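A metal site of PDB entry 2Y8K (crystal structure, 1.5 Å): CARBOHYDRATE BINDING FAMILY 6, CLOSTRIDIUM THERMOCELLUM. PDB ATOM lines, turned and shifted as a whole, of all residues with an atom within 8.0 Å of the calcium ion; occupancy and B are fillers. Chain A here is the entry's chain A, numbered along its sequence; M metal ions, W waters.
The backbone carbonyl oxygen of Asp 376 sits at hydrogen-bond distance from the backbone NH of Gly 390, at 2.9 Å.
The side-chain carboxylate of Asp 376 sits at hydrogen-bond distance from the backbone NH of Val 365, at 2.9 Å.
The side-chain carboxylate (OD2) of Asp 359 sits close to the backbone NH (N) of Asp 361 (3.1 Å).
The side-chain carboxylate (OE1) of Glu 396 lies close to the backbone NH (N) of Ser 393, at 3.0 Å.
OE2 of Glu 396 lies close to N of Thr 360 (2.8 Å).
Within 4 Å of the calcium ion: Asp 359, Asp 376, Trp 391 and Glu 396.
Along chain A the residues within 4 Å of the calcium ion span positions 359 to 396.
The calcium ion is bound by the side-chain carboxylate (OD2) of Asp 376 (2.3 Å), the backbone carbonyl oxygen (O) of Trp 391 (2.4 Å), the side-chain carboxylate (OD1) of Asp 359 (2.4 Å), water W2 (2.5 Å), the side-chain carboxylate (OE1) of Glu 396 (2.6 Å), water W1 (2.6 Å), the side-chain carboxylate (OE2) of Glu 396 (2.6 Å) and the side-chain carboxylate (OD2) of Asp 359 (2.9 Å).
The calcium ion has eight donor atoms within binding distance.
Water W2 lies within hydrogen-bond range of O of Gly 390 (2.7 Å) and N of Asp 376 (3.2 Å).
Water W1 bridges the side-chain hydroxyl of Thr 360 (2.8 Å) and the side-chain hydroxyl of Ser 393 (2.8 Å).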
ATOM      1  N   TYR A 358      25.691  17.974 -14.282  1.00  0.00           N
ATOM      2  CA  TYR A 358      24.755  18.281 -13.189  1.00  0.00           C
ATOM      3  C   TYR A 358      24.724  19.781 -12.999  1.00  0.00           C
ATOM      4  O   TYR A 358      25.765  20.429 -12.847  1.00  0.00           O
ATOM      5  CB  TYR A 358      25.104  17.572 -11.881  1.00  0.00           C
ATOM      6  CG  TYR A 358      24.242  18.051 -10.738  1.00  0.00           C
ATOM      7  CD1 TYR A 358      22.888  17.772 -10.731  1.00  0.00           C
ATOM      8  CD2 TYR A 358      24.782  18.783  -9.675  1.00  0.00           C
ATOM      9  CE1 TYR A 358      22.059  18.224  -9.693  1.00  0.00           C
ATOM     10  CE2 TYR A 358      23.960  19.231  -8.632  1.00  0.00           C
ATOM     11  CZ  TYR A 358      22.620  18.950  -8.664  1.00  0.00           C
ATOM     12  OH  TYR A 358      21.815  19.402  -7.623  1.00  0.00           O
ATOM     13  N   ASP A 359      23.511  20.350 -13.044  1.00  0.00           N
ATOM     14  CA  ASP A 359      23.313  21.754 -12.809  1.00  0.00           C
ATOM     15  C   ASP A 359      22.226  21.942 -11.751  1.00  0.00           C
ATOM     16  O   ASP A 359      21.216  21.227 -11.766  1.00  0.00           O
ATOM     17  CB  ASP A 359      22.894  22.509 -14.061  1.00  0.00           C
ATOM     18  CG  ASP A 359      23.308  23.952 -14.004  1.00  0.00           C
ATOM     19  OD1 ASP A 359      24.443  24.299 -14.405  1.00  0.00           O
ATOM     20  OD2 ASP A 359      22.511  24.792 -13.501  1.00  0.00           O
ATOM     21  N   THR A 360      22.462  22.892 -10.852  1.00  0.00           N
ATOM     22  CA  THR A 360      21.531  23.175  -9.764  1.00  0.00           C
ATOM     23  C   THR A 360      20.246  23.882 -10.196  1.00  0.00           C
ATOM     24  O   THR A 360      19.279  23.902  -9.426  1.00  0.00           O
ATOM     25  CB  THR A 360      22.203  24.011  -8.650  1.00  0.00           C
ATOM     26  OG1 THR A 360      22.629  25.286  -9.160  1.00  0.00           O
ATOM     27  CG2 THR A 360      23.404  23.272  -8.062  1.00  0.00           C
ATOM     28  N   ASP A 361      20.235  24.451 -11.392  1.00  0.00           N
ATOM     29  CA  ASP A 361      19.028  25.053 -12.007  1.00  0.00           C
ATOM     30  C   ASP A 361      18.687  24.182 -13.209  1.00  0.00           C
ATOM     31  O   ASP A 361      19.514  24.024 -14.098  1.00  0.00           O
ATOM     32  CB  ASP A 361      19.343  26.472 -12.504  1.00  0.00           C
ATOM     33  CG  ASP A 361      18.898  27.553 -11.568  1.00  0.00           C
ATOM     34  OD1 ASP A 361      17.684  27.585 -11.283  1.00  0.00           O
ATOM     35  OD2 ASP A 361      19.760  28.389 -11.180  1.00  0.00           O
ATOM     36  N   SER A 362      17.476  23.630 -13.256  1.00  0.00           N
ATOM     37  CA  SER A 362      17.066  22.829 -14.406  1.00  0.00           C
ATOM     38  C   SER A 362      17.082  23.613 -15.718  1.00  0.00           C
ATOM     39  O   SER A 362      17.295  23.042 -16.778  1.00  0.00           O
ATOM     40  CB  SER A 362      15.698  22.188 -14.154  1.00  0.00           C
ATOM     41  OG  SER A 362      14.708  23.180 -13.984  1.00  0.00           O
ATOM     42  N   VAL A 363      16.863  24.929 -15.646  1.00  0.00           N
ATOM     43  CA  VAL A 363      16.908  25.808 -16.803  1.00  0.00           C
ATOM     44  C   VAL A 363      18.319  26.341 -17.021  1.00  0.00           C
ATOM     45  O   VAL A 363      19.046  26.576 -16.041  1.00  0.00           O
ATOM     46  CB  VAL A 363      15.954  26.998 -16.587  1.00  0.00           C
ATOM     47  CG1 VAL A 363      16.107  28.044 -17.672  1.00  0.00           C
ATOM     48  CG2 VAL A 363      14.515  26.465 -16.480  1.00  0.00           C
ATOM     49  N   ASN A 364      18.712  26.493 -18.277  1.00  0.00           N
ATOM     50  CA  ASN A 364      19.908  27.207 -18.682  1.00  0.00           C
ATOM     51  C   ASN A 364      19.649  28.693 -18.473  1.00  0.00           C
ATOM     52  O   ASN A 364      19.034  29.367 -19.310  1.00  0.00           O
ATOM     53  CB  ASN A 364      20.256  26.895 -20.155  1.00  0.00           C
ATOM     54  CG  ASN A 364      21.336  27.769 -20.717  1.00  0.00           C
ATOM     55  OD1 ASN A 364      21.851  28.720 -20.087  1.00  0.00           O
ATOM     56  ND2 ASN A 364      21.707  27.451 -21.962  1.00  0.00           N
ATOM     57  N   VAL A 365      20.145  29.221 -17.354  1.00  0.00           N
ATOM     58  CA  VAL A 365      19.765  30.616 -17.014  1.00  0.00           C
ATOM     59  C   VAL A 365      20.409  31.676 -17.874  1.00  0.00           C
ATOM     60  O   VAL A 365      19.915  32.802 -17.912  1.00  0.00           O
ATOM     61  CB  VAL A 365      19.955  30.937 -15.500  1.00  0.00           C
ATOM     62  CG1 VAL A 365      19.191  29.950 -14.642  1.00  0.00           C
ATOM     63  CG2 VAL A 365      21.436  31.013 -15.133  1.00  0.00           C
ATOM     64  N   GLY A 374      20.430  22.019 -19.295  1.00  0.00           N
ATOM     65  CA  GLY A 374      20.476  22.658 -17.995  1.00  0.00           C
ATOM     66  C   GLY A 374      21.738  23.425 -17.647  1.00  0.00           C
ATOM     67  O   GLY A 374      21.731  24.222 -16.691  1.00  0.00           O
ATOM     68  N   VAL A 375      22.825  23.245 -18.398  1.00  0.00           N
ATOM     69  CA  VAL A 375      24.064  23.960 -18.091  1.00  0.00           C
ATOM     70  C   VAL A 375      23.850  25.424 -18.396  1.00  0.00           C
ATOM     71  O   VAL A 375      23.201  25.755 -19.382  1.00  0.00           O
ATOM     72  CB  VAL A 375      25.262  23.367 -18.891  1.00  0.00           C
ATOM     73  CG1 VAL A 375      26.541  24.166 -18.621  1.00  0.00           C
ATOM     74  CG2 VAL A 375      25.436  21.904 -18.527  1.00  0.00           C
ATOM     75  N   ASP A 376      24.357  26.330 -17.561  1.00  0.00           N
ATOM     76  CA  ASP A 376      24.140  27.765 -17.768  1.00  0.00           C
ATOM     77  C   ASP A 376      25.233  28.334 -18.672  1.00  0.00           C
ATOM     78  O   ASP A 376      26.425  28.241 -18.345  1.00  0.00           O
ATOM     79  CB  ASP A 376      24.087  28.473 -16.411  1.00  0.00           C
ATOM     80  CG  ASP A 376      23.149  27.845 -15.450  1.00  0.00           C
ATOM     81  OD1 ASP A 376      21.985  27.594 -15.830  1.00  0.00           O
ATOM     82  OD2 ASP A 376      23.535  27.577 -14.268  1.00  0.00           O
ATOM     83  N   ILE A 377      24.849  28.892 -19.809  1.00  0.00           N
ATOM     84  CA  ILE A 377      25.761  29.277 -20.861  1.00  0.00           C
ATOM     85  C   ILE A 377      25.475  30.707 -21.311  1.00  0.00           C
ATOM     86  O   ILE A 377      24.322  31.038 -21.549  1.00  0.00           O
ATOM     87  CB  ILE A 377      25.659  28.319 -22.091  1.00  0.00           C
ATOM     88  CG1 ILE A 377      25.788  26.859 -21.660  1.00  0.00           C
ATOM     89  CG2 ILE A 377      26.729  28.671 -23.148  1.00  0.00           C
ATOM     90  CD1 ILE A 377      25.480  25.860 -22.772  1.00  0.00           C
ATOM     91  N   VAL A 389      30.618  28.677 -20.062  1.00  0.00           N
ATOM     92  CA  VAL A 389      29.766  28.191 -19.015  1.00  0.00           C
ATOM     93  C   VAL A 389      29.915  29.166 -17.842  1.00  0.00           C
ATOM     94  O   VAL A 389      31.030  29.560 -17.482  1.00  0.00           O
ATOM     95  CB  VAL A 389      30.145  26.748 -18.613  1.00  0.00           C
ATOM     96  CG1 VAL A 389      29.313  26.283 -17.392  1.00  0.00           C
ATOM     97  CG2 VAL A 389      29.954  25.807 -19.853  1.00  0.00           C
ATOM     98  N   GLY A 390      28.772  29.595 -17.310  1.00  0.00           N
ATOM     99  CA  GLY A 390      28.710  30.521 -16.186  1.00  0.00           C
ATOM    100  C   GLY A 390      27.798  30.004 -15.111  1.00  0.00           C
ATOM    101  O   GLY A 390      27.272  28.892 -15.175  1.00  0.00           O
ATOM    102  N   TRP A 391      27.545  30.835 -14.097  1.00  0.00           N
ATOM    103  CA  TRP A 391      26.735  30.400 -12.963  1.00  0.00           C
ATOM    104  C   TRP A 391      27.108  28.977 -12.520  1.00  0.00           C
ATOM    105  O   TRP A 391      26.249  28.106 -12.333  1.00  0.00           O
ATOM    106  CB  TRP A 391      25.233  30.492 -13.277  1.00  0.00           C
ATOM    107  CG  TRP A 391      24.778  31.854 -13.758  1.00  0.00           C
ATOM    108  CD1 TRP A 391      24.262  32.869 -12.973  1.00  0.00           C
ATOM    109  CD2 TRP A 391      24.798  32.356 -15.101  1.00  0.00           C
ATOM    110  NE1 TRP A 391      23.956  33.976 -13.768  1.00  0.00           N
ATOM    111  CE2 TRP A 391      24.283  33.681 -15.068  1.00  0.00           C
ATOM    112  CE3 TRP A 391      25.211  31.823 -16.330  1.00  0.00           C
ATOM    113  CZ2 TRP A 391      24.156  34.457 -16.217  1.00  0.00           C
ATOM    114  CZ3 TRP A 391      25.070  32.594 -17.463  1.00  0.00           C
ATOM    115  CH2 TRP A 391      24.555  33.915 -17.394  1.00  0.00           C
ATOM    116  N   ILE A 392      28.408  28.761 -12.319  1.00  0.00           N
ATOM    117  CA  ILE A 392      28.937  27.481 -11.890  1.00  0.00           C
ATOM    118  C   ILE A 392      28.878  27.417 -10.376  1.00  0.00           C
ATOM    119  O   ILE A 392      29.468  28.244  -9.678  1.00  0.00           O
ATOM    120  CB  ILE A 392      30.375  27.272 -12.375  1.00  0.00           C
ATOM    121  CG1 ILE A 392      30.429  27.296 -13.909  1.00  0.00           C
ATOM    122  CG2 ILE A 392      30.869  25.903 -11.881  1.00  0.00           C
ATOM    123  CD1 ILE A 392      31.830  27.095 -14.561  1.00  0.00           C
ATOM    124  N   SER A 393      28.107  26.462  -9.883  1.00  0.00           N
ATOM    125  CA  SER A 393      27.827  26.304  -8.475  1.00  0.00           C
ATOM    126  C   SER A 393      28.560  25.089  -7.898  1.00  0.00           C
ATOM    127  O   SER A 393      28.779  24.085  -8.605  1.00  0.00           O
ATOM    128  CB  SER A 393      26.328  26.155  -8.224  1.00  0.00           C
ATOM    129  OG  SER A 393      25.619  27.298  -8.715  1.00  0.00           O
ATOM    130  N   GLU A 394      28.950  25.182  -6.624  1.00  0.00           N
ATOM    131  CA  GLU A 394      29.570  24.050  -5.941  1.00  0.00           C
ATOM    132  C   GLU A 394      28.751  22.776  -6.107  1.00  0.00           C
ATOM    133  O   GLU A 394      27.541  22.801  -5.889  1.00  0.00           O
ATOM    134  CB  GLU A 394      29.736  24.316  -4.431  1.00  0.00           C
ATOM    135  CG  GLU A 394      30.602  23.320  -3.764  1.00  0.00           C
ATOM    136  CD  GLU A 394      30.854  23.541  -2.277  1.00  0.00           C
ATOM    137  OE1 GLU A 394      30.872  24.708  -1.856  1.00  0.00           O
ATOM    138  OE2 GLU A 394      31.070  22.534  -1.565  1.00  0.00           O
ATOM    139  N   GLU A 396      28.391  21.134  -8.984  1.00  0.00           N
ATOM    140  CA  GLU A 396      28.065  20.939 -10.402  1.00  0.00           C
ATOM    141  C   GLU A 396      29.211  20.181 -11.051  1.00  0.00           C
ATOM    142  O   GLU A 396      30.300  20.114 -10.519  1.00  0.00           O
ATOM    143  CB  GLU A 396      27.751  22.250 -11.121  1.00  0.00           C
ATOM    144  CG  GLU A 396      26.459  22.884 -10.610  1.00  0.00           C
ATOM    145  CD  GLU A 396      26.017  24.132 -11.358  1.00  0.00           C
ATOM    146  OE1 GLU A 396      26.816  24.827 -12.014  1.00  0.00           O
ATOM    147  OE2 GLU A 396      24.793  24.415 -11.301  1.00  0.00           O
ATOM    148  N   TRP A 397      28.923  19.577 -12.185  1.00  0.00           N
ATOM    149  CA  TRP A 397      29.938  18.873 -12.947  1.00  0.00           C
ATOM    150  C   TRP A 397      29.557  18.780 -14.405  1.00  0.00           C
ATOM    151  O   TRP A 397      28.401  18.926 -14.767  1.00  0.00           O
ATOM    152  CB  TRP A 397      30.224  17.497 -12.364  1.00  0.00           C
ATOM    153  CG  TRP A 397      29.043  16.608 -12.026  1.00  0.00           C
ATOM    154  CD1 TRP A 397      28.430  16.488 -10.827  1.00  0.00           C
ATOM    155  CD2 TRP A 397      28.389  15.692 -12.902  1.00  0.00           C
ATOM    156  NE1 TRP A 397      27.452  15.544 -10.877  1.00  0.00           N
ATOM    157  CE2 TRP A 397      27.401  15.025 -12.142  1.00  0.00           C
ATOM    158  CE3 TRP A 397      28.582  15.336 -14.237  1.00  0.00           C
ATOM    159  CZ2 TRP A 397      26.568  14.040 -12.712  1.00  0.00           C
ATOM    160  CZ3 TRP A 397      27.742  14.342 -14.785  1.00  0.00           C
ATOM    161  CH2 TRP A 397      26.771  13.723 -14.035  1.00  0.00           C
ATOM    162  N   LEU A 398      30.563  18.599 -15.265  1.00  0.00           N
ATOM    163  CA  LEU A 398      30.432  18.564 -16.723  1.00  0.00           C
ATOM    164  C   LEU A 398      31.299  17.411 -17.223  1.00  0.00           C
ATOM    165  O   LEU A 398      32.456  17.271 -16.802  1.00  0.00           O
ATOM    166  CB  LEU A 398      30.952  19.863 -17.334  1.00  0.00           C
ATOM    167  CG  LEU A 398      30.258  21.129 -16.855  1.00  0.00           C
ATOM    168  CD1 LEU A 398      31.130  22.378 -17.066  1.00  0.00           C
ATOM    169  CD2 LEU A 398      28.908  21.298 -17.563  1.00  0.00           C
HETATM  170 CA    CA M   1      24.974  26.246 -13.112  1.00  0.00          CA
HETATM  171  O   HOH W   1      23.847  27.048 -10.932  1.00  0.00           O
HETATM  172  O   HOH W   2      26.450  26.275 -15.130  1.00  0.00           O
